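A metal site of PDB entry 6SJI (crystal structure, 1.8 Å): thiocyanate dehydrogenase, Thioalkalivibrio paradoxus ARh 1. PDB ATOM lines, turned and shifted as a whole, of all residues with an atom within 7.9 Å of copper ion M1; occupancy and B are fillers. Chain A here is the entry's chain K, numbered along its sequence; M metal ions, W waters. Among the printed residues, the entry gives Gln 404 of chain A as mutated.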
ATOM      1  N   LYS A  25      19.413   1.774  -0.057  1.00  0.00           N
ATOM      2  CA  LYS A  25      18.301   1.018  -0.698  1.00  0.00           C
ATOM      3  C   LYS A  25      17.493   1.928  -1.645  1.00  0.00           C
ATOM      4  O   LYS A  25      18.089   2.444  -2.617  1.00  0.00           O
ATOM      5  CB  LYS A  25      17.419   0.365   0.382  1.00  0.00           C
ATOM      6  CG  LYS A  25      16.448  -0.743  -0.021  1.00  0.00           C
ATOM      7  CD  LYS A  25      17.093  -2.107  -0.043  1.00  0.00           C
ATOM      8  CE  LYS A  25      15.991  -3.073  -0.437  1.00  0.00           C
ATOM      9  NZ  LYS A  25      16.372  -4.518  -0.548  1.00  0.00           N
ATOM     10  N   ILE A  55      18.876   0.559  -6.473  1.00  0.00           N
ATOM     11  CA  ILE A  55      18.551   0.037  -5.094  1.00  0.00           C
ATOM     12  C   ILE A  55      19.902  -0.395  -4.511  1.00  0.00           C
ATOM     13  O   ILE A  55      20.331  -1.498  -4.789  1.00  0.00           O
ATOM     14  CB  ILE A  55      17.535  -1.109  -5.123  1.00  0.00           C
ATOM     15  CG1 ILE A  55      16.206  -0.637  -5.814  1.00  0.00           C
ATOM     16  CG2 ILE A  55      17.276  -1.676  -3.703  1.00  0.00           C
ATOM     17  CD1 ILE A  55      15.204  -1.758  -6.109  1.00  0.00           C
ATOM     18  N   MET A  56      20.570   0.497  -3.735  1.00  0.00           N
ATOM     19  CA  MET A  56      21.922   0.216  -3.221  1.00  0.00           C
ATOM     20  C   MET A  56      21.772  -0.697  -2.026  1.00  0.00           C
ATOM     21  O   MET A  56      21.070  -0.345  -1.032  1.00  0.00           O
ATOM     22  CB  MET A  56      22.550   1.566  -2.789  1.00  0.00           C
ATOM     23  CG  MET A  56      22.614   2.547  -3.968  1.00  0.00           C
ATOM     24  SD  MET A  56      23.783   2.001  -5.212  1.00  0.00           S
ATOM     25  CE  MET A  56      25.370   2.432  -4.524  1.00  0.00           C
ATOM     26  N   HIS A  57      22.302  -1.897  -2.120  1.00  0.00           N
ATOM     27  CA  HIS A  57      21.806  -2.922  -1.225  1.00  0.00           C
ATOM     28  C   HIS A  57      22.732  -3.332  -0.066  1.00  0.00           C
ATOM     29  O   HIS A  57      22.657  -2.775   1.004  1.00  0.00           O
ATOM     30  CB  HIS A  57      21.338  -4.157  -2.015  1.00  0.00           C
ATOM     31  CG  HIS A  57      20.454  -5.044  -1.199  1.00  0.00           C
ATOM     32  ND1 HIS A  57      20.210  -6.369  -1.513  1.00  0.00           N
ATOM     33  CD2 HIS A  57      19.761  -4.789  -0.072  1.00  0.00           C
ATOM     34  CE1 HIS A  57      19.353  -6.875  -0.631  1.00  0.00           C
ATOM     35  NE2 HIS A  57      19.045  -5.923   0.251  1.00  0.00           N
ATOM     36  N   HIS A  58      23.615  -4.304  -0.283  1.00  0.00           N
ATOM     37  CA  HIS A  58      24.487  -4.731   0.776  1.00  0.00           C
ATOM     38  C   HIS A  58      25.903  -4.219   0.525  1.00  0.00           C
ATOM     39  O   HIS A  58      26.255  -3.799  -0.600  1.00  0.00           O
ATOM     40  CB  HIS A  58      24.437  -6.284   0.959  1.00  0.00           C
ATOM     41  CG  HIS A  58      23.176  -6.759   1.617  1.00  0.00           C
ATOM     42  ND1 HIS A  58      22.896  -6.501   2.947  1.00  0.00           N
ATOM     43  CD2 HIS A  58      22.120  -7.468   1.127  1.00  0.00           C
ATOM     44  CE1 HIS A  58      21.707  -7.019   3.259  1.00  0.00           C
ATOM     45  NE2 HIS A  58      21.218  -7.612   2.177  1.00  0.00           N
ATOM     46  N   GLN A  78      20.084  -4.144  -6.326  1.00  0.00           N
ATOM     47  CA  GLN A  78      18.956  -4.954  -6.782  1.00  0.00           C
ATOM     48  C   GLN A  78      18.146  -4.170  -7.787  1.00  0.00           C
ATOM     49  O   GLN A  78      18.226  -2.938  -7.869  1.00  0.00           O
ATOM     50  CB  GLN A  78      17.990  -5.345  -5.656  1.00  0.00           C
ATOM     51  CG  GLN A  78      18.633  -6.414  -4.810  1.00  0.00           C
ATOM     52  CD  GLN A  78      17.774  -6.828  -3.678  1.00  0.00           C
ATOM     53  OE1 GLN A  78      17.214  -5.980  -2.976  1.00  0.00           O
ATOM     54  NE2 GLN A  78      17.742  -8.130  -3.413  1.00  0.00           N
ATOM     55  N   ASN A  82      12.083  -6.233  -7.563  1.00  0.00           N
ATOM     56  CA  ASN A  82      12.440  -5.744  -6.171  1.00  0.00           C
ATOM     57  C   ASN A  82      11.978  -4.293  -5.929  1.00  0.00           C
ATOM     58  O   ASN A  82      11.808  -3.882  -4.787  1.00  0.00           O
ATOM     59  CB  ASN A  82      13.937  -5.822  -5.862  1.00  0.00           C
ATOM     60  CG  ASN A  82      14.422  -7.243  -5.755  1.00  0.00           C
ATOM     61  OD1 ASN A  82      14.126  -7.955  -4.775  1.00  0.00           O
ATOM     62  ND2 ASN A  82      15.223  -7.703  -6.765  1.00  0.00           N
ATOM     63  N   TYR A  86       8.049  -2.810  -1.726  1.00  0.00           N
ATOM     64  CA  TYR A  86       8.091  -1.999  -0.489  1.00  0.00           C
ATOM     65  C   TYR A  86       6.849  -1.071  -0.460  1.00  0.00           C
ATOM     66  O   TYR A  86       5.960  -1.103  -1.335  1.00  0.00           O
ATOM     67  CB  TYR A  86       9.481  -1.320  -0.198  1.00  0.00           C
ATOM     68  CG  TYR A  86      10.621  -2.353  -0.090  1.00  0.00           C
ATOM     69  CD1 TYR A  86      11.240  -2.872  -1.240  1.00  0.00           C
ATOM     70  CD2 TYR A  86      11.034  -2.889   1.169  1.00  0.00           C
ATOM     71  CE1 TYR A  86      12.255  -3.872  -1.159  1.00  0.00           C
ATOM     72  CE2 TYR A  86      12.031  -3.880   1.259  1.00  0.00           C
ATOM     73  CZ  TYR A  86      12.609  -4.391   0.118  1.00  0.00           C
ATOM     74  OH  TYR A  86      13.620  -5.355   0.180  1.00  0.00           O
ATOM     75  N   GLY A 126      22.967 -10.101  -6.009  1.00  0.00           N
ATOM     76  CA  GLY A 126      22.301  -8.936  -5.414  1.00  0.00           C
ATOM     77  C   GLY A 126      21.921  -9.030  -3.946  1.00  0.00           C
ATOM     78  O   GLY A 126      21.189  -8.124  -3.445  1.00  0.00           O
ATOM     79  N   VAL A 127      22.372 -10.086  -3.247  1.00  0.00           N
ATOM     80  CA  VAL A 127      22.165 -10.136  -1.768  1.00  0.00           C
ATOM     81  C   VAL A 127      23.467  -9.879  -0.970  1.00  0.00           C
ATOM     82  O   VAL A 127      24.128  -8.878  -1.219  1.00  0.00           O
ATOM     83  CB  VAL A 127      21.297 -11.376  -1.328  1.00  0.00           C
ATOM     84  CG1 VAL A 127      20.703 -11.137   0.063  1.00  0.00           C
ATOM     85  CG2 VAL A 127      20.156 -11.617  -2.353  1.00  0.00           C
ATOM     86  N   HIS A 128      23.847 -10.697   0.027  1.00  0.00           N
ATOM     87  CA  HIS A 128      24.865 -10.234   0.985  1.00  0.00           C
ATOM     88  C   HIS A 128      26.273 -10.182   0.418  1.00  0.00           C
ATOM     89  O   HIS A 128      26.649 -11.045  -0.401  1.00  0.00           O
ATOM     90  CB  HIS A 128      24.906 -11.025   2.302  1.00  0.00           C
ATOM     91  CG  HIS A 128      23.688 -10.831   3.138  1.00  0.00           C
ATOM     92  ND1 HIS A 128      23.532  -9.790   4.021  1.00  0.00           N
ATOM     93  CD2 HIS A 128      22.539 -11.562   3.227  1.00  0.00           C
ATOM     94  CE1 HIS A 128      22.385  -9.911   4.669  1.00  0.00           C
ATOM     95  NE2 HIS A 128      21.765 -10.981   4.213  1.00  0.00           N
ATOM     96  N   GLU A 210      13.883 -10.911  -4.326  1.00  0.00           N
ATOM     97  CA  GLU A 210      14.413 -11.620  -3.179  1.00  0.00           C
ATOM     98  C   GLU A 210      13.233 -11.813  -2.211  1.00  0.00           C
ATOM     99  O   GLU A 210      12.448 -10.845  -1.980  1.00  0.00           O
ATOM    100  CB  GLU A 210      15.557 -10.772  -2.551  1.00  0.00           C
ATOM    101  CG  GLU A 210      15.993 -11.279  -1.180  1.00  0.00           C
ATOM    102  CD  GLU A 210      16.810 -10.269  -0.368  1.00  0.00           C
ATOM    103  OE1 GLU A 210      17.010  -9.057  -0.767  1.00  0.00           O
ATOM    104  OE2 GLU A 210      17.251 -10.665   0.746  1.00  0.00           O
ATOM    105  N   LEU A 211      13.128 -13.005  -1.597  1.00  0.00           N
ATOM    106  CA  LEU A 211      11.987 -13.249  -0.707  1.00  0.00           C
ATOM    107  C   LEU A 211      12.067 -12.297   0.466  1.00  0.00           C
ATOM    108  O   LEU A 211      13.161 -12.031   0.973  1.00  0.00           O
ATOM    109  CB  LEU A 211      12.009 -14.688  -0.197  1.00  0.00           C
ATOM    110  CG  LEU A 211      11.842 -15.746  -1.297  1.00  0.00           C
ATOM    111  CD1 LEU A 211      11.821 -17.091  -0.598  1.00  0.00           C
ATOM    112  CD2 LEU A 211      10.564 -15.537  -2.114  1.00  0.00           C
ATOM    113  N   HIS A 359      19.952 -10.143  11.654  1.00  0.00           N
ATOM    114  CA  HIS A 359      21.320  -9.594  11.726  1.00  0.00           C
ATOM    115  C   HIS A 359      21.922  -9.709  13.119  1.00  0.00           C
ATOM    116  O   HIS A 359      21.195  -9.672  14.125  1.00  0.00           O
ATOM    117  CB  HIS A 359      21.302  -8.104  11.325  1.00  0.00           C
ATOM    118  CG  HIS A 359      20.734  -7.896   9.966  1.00  0.00           C
ATOM    119  ND1 HIS A 359      21.415  -8.260   8.817  1.00  0.00           N
ATOM    120  CD2 HIS A 359      19.497  -7.482   9.584  1.00  0.00           C
ATOM    121  CE1 HIS A 359      20.633  -8.019   7.772  1.00  0.00           C
ATOM    122  NE2 HIS A 359      19.463  -7.569   8.214  1.00  0.00           N
ATOM    123  N   GLN A 404      17.059  -2.717  10.989  1.00  0.00           N
ATOM    124  CA  GLN A 404      17.818  -3.422   9.948  1.00  0.00           C
ATOM    125  C   GLN A 404      19.161  -3.916  10.519  1.00  0.00           C
ATOM    126  O   GLN A 404      19.153  -4.862  11.274  1.00  0.00           O
ATOM    127  CB  GLN A 404      17.941  -2.575   8.656  1.00  0.00           C
ATOM    128  CG  GLN A 404      16.587  -2.434   7.990  1.00  0.00           C
ATOM    129  CD  GLN A 404      16.255  -3.728   7.274  1.00  0.00           C
ATOM    130  OE1 GLN A 404      17.155  -4.481   6.898  1.00  0.00           O
ATOM    131  NE2 GLN A 404      14.963  -3.993   7.044  1.00  0.00           N
ATOM    132  N   GLN A 423      11.362   1.920   3.892  1.00  0.00           N
ATOM    133  CA  GLN A 423      11.626   2.717   2.654  1.00  0.00           C
ATOM    134  C   GLN A 423      10.664   3.907   2.568  1.00  0.00           C
ATOM    135  O   GLN A 423      10.711   4.610   1.539  1.00  0.00           O
ATOM    136  CB  GLN A 423      11.521   1.849   1.316  1.00  0.00           C
ATOM    137  CG  GLN A 423      12.446   0.558   1.327  1.00  0.00           C
ATOM    138  CD  GLN A 423      13.885   0.923   1.696  1.00  0.00           C
ATOM    139  OE1 GLN A 423      14.505   1.813   1.094  1.00  0.00           O
ATOM    140  NE2 GLN A 423      14.377   0.351   2.773  1.00  0.00           N
ATOM    141  N   GLY A 448      17.433   4.233   3.296  1.00  0.00           N
ATOM    142  CA  GLY A 448      16.677   2.981   3.617  1.00  0.00           C
ATOM    143  C   GLY A 448      17.546   1.784   3.926  1.00  0.00           C
ATOM    144  O   GLY A 448      17.128   0.669   3.592  1.00  0.00           O
ATOM    145  N   HIS A 449      18.726   2.040   4.532  1.00  0.00           N
ATOM    146  CA  HIS A 449      19.811   1.090   4.784  1.00  0.00           C
ATOM    147  C   HIS A 449      19.348  -0.315   5.070  1.00  0.00           C
ATOM    148  O   HIS A 449      18.550  -0.577   5.996  1.00  0.00           O
ATOM    149  CB  HIS A 449      20.738   1.561   5.999  1.00  0.00           C
ATOM    150  CG  HIS A 449      20.326   2.880   6.598  1.00  0.00           C
ATOM    151  ND1 HIS A 449      19.136   3.050   7.281  1.00  0.00           N
ATOM    152  CD2 HIS A 449      20.957   4.082   6.635  1.00  0.00           C
ATOM    153  CE1 HIS A 449      19.079   4.291   7.751  1.00  0.00           C
ATOM    154  NE2 HIS A 449      20.177   4.928   7.376  1.00  0.00           N
ATOM    155  N   HIS A 450      19.854  -1.238   4.260  1.00  0.00           N
ATOM    156  CA  HIS A 450      19.766  -2.643   4.603  1.00  0.00           C
ATOM    157  C   HIS A 450      21.154  -3.184   4.917  1.00  0.00           C
ATOM    158  O   HIS A 450      21.352  -4.419   4.989  1.00  0.00           O
ATOM    159  CB  HIS A 450      19.174  -3.449   3.449  1.00  0.00           C
ATOM    160  CG  HIS A 450      17.679  -3.460   3.471  1.00  0.00           C
ATOM    161  ND1 HIS A 450      16.919  -4.386   2.777  1.00  0.00           N
ATOM    162  CD2 HIS A 450      16.796  -2.617   4.080  1.00  0.00           C
ATOM    163  CE1 HIS A 450      15.625  -4.137   2.975  1.00  0.00           C
ATOM    164  NE2 HIS A 450      15.518  -3.054   3.738  1.00  0.00           N
ATOM    165  N   ASP A 451      22.102  -2.282   5.135  1.00  0.00           N
ATOM    166  CA  ASP A 451      23.417  -2.731   5.603  1.00  0.00           C
ATOM    167  C   ASP A 451      24.055  -1.556   6.280  1.00  0.00           C
ATOM    168  O   ASP A 451      23.639  -0.394   6.083  1.00  0.00           O
ATOM    169  CB  ASP A 451      24.255  -3.251   4.475  1.00  0.00           C
ATOM    170  CG  ASP A 451      25.071  -4.535   4.896  1.00  0.00           C
ATOM    171  OD1 ASP A 451      25.467  -4.679   6.077  1.00  0.00           O
ATOM    172  OD2 ASP A 451      25.286  -5.424   4.073  1.00  0.00           O
HETATM  173 CU    CU M   1      17.527  -5.622   1.440  1.00  0.00          CU
HETATM  174 CU    CU M   2      20.193 -11.906   4.885  1.00  0.00          CU
HETATM  175  O   HOH W   1      17.948  -6.781   2.952  1.00  0.00           O
HETATM  176  O   HOH W   2      16.274  -7.118   0.986  1.00  0.00           O
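The backbone carbonyl oxygen (O) of His 450 sits close to a ring nitrogen (ND1) of His 58, 3.3 Å away. NE2 of His 450 lies within hydrogen-bond range of NE2 of Gln 404, 3.5 Å away. A ring nitrogen (NE2) of His 57 sits close to a ring nitrogen (NE2) of His 58 (3.4 Å). A ring nitrogen (ND1) of His 57 lies close to the side-chain amide oxygen (OE1) of Gln 78. A ring nitrogen (ND1) of His 57 is in hydrogen-bond range of the backbone carbonyl oxygen of Gly 126, 2.8 Å away. The side-chain amino group of Lys 25 sits close to the side-chain hydroxyl of Tyr 86 (3.0 Å). The side-chain amide oxygen (OE1) of Gln 78 lies close to the side-chain amino group (NZ) of Lys 25 (3.0 Å). O of Met 56 sits at hydrogen-bond distance from N of Lys 25 (2.9 Å).
The nearest printed residue that does not touch copper ion M1 is Tyr 86 (4.1 Å).
ND1 of His 450 is bound to copper ion M1 (1.9 Å). Water W1 binds copper ion M1 (2.0 Å). Copper ion M1 is bound by a ring nitrogen (NE2) of His 57 (2.0 Å). Water W2 is bound to copper ion M1, 2.0 Å away. The side-chain amino group (NZ) of Lys 25 binds copper ion M1 (2.6 Å). Copper ion M1 has five donor atoms within binding distance.
Water W2 bridges OE1 of Glu 210 (2.7 Å) and OH of Tyr 86 (3.3 Å).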
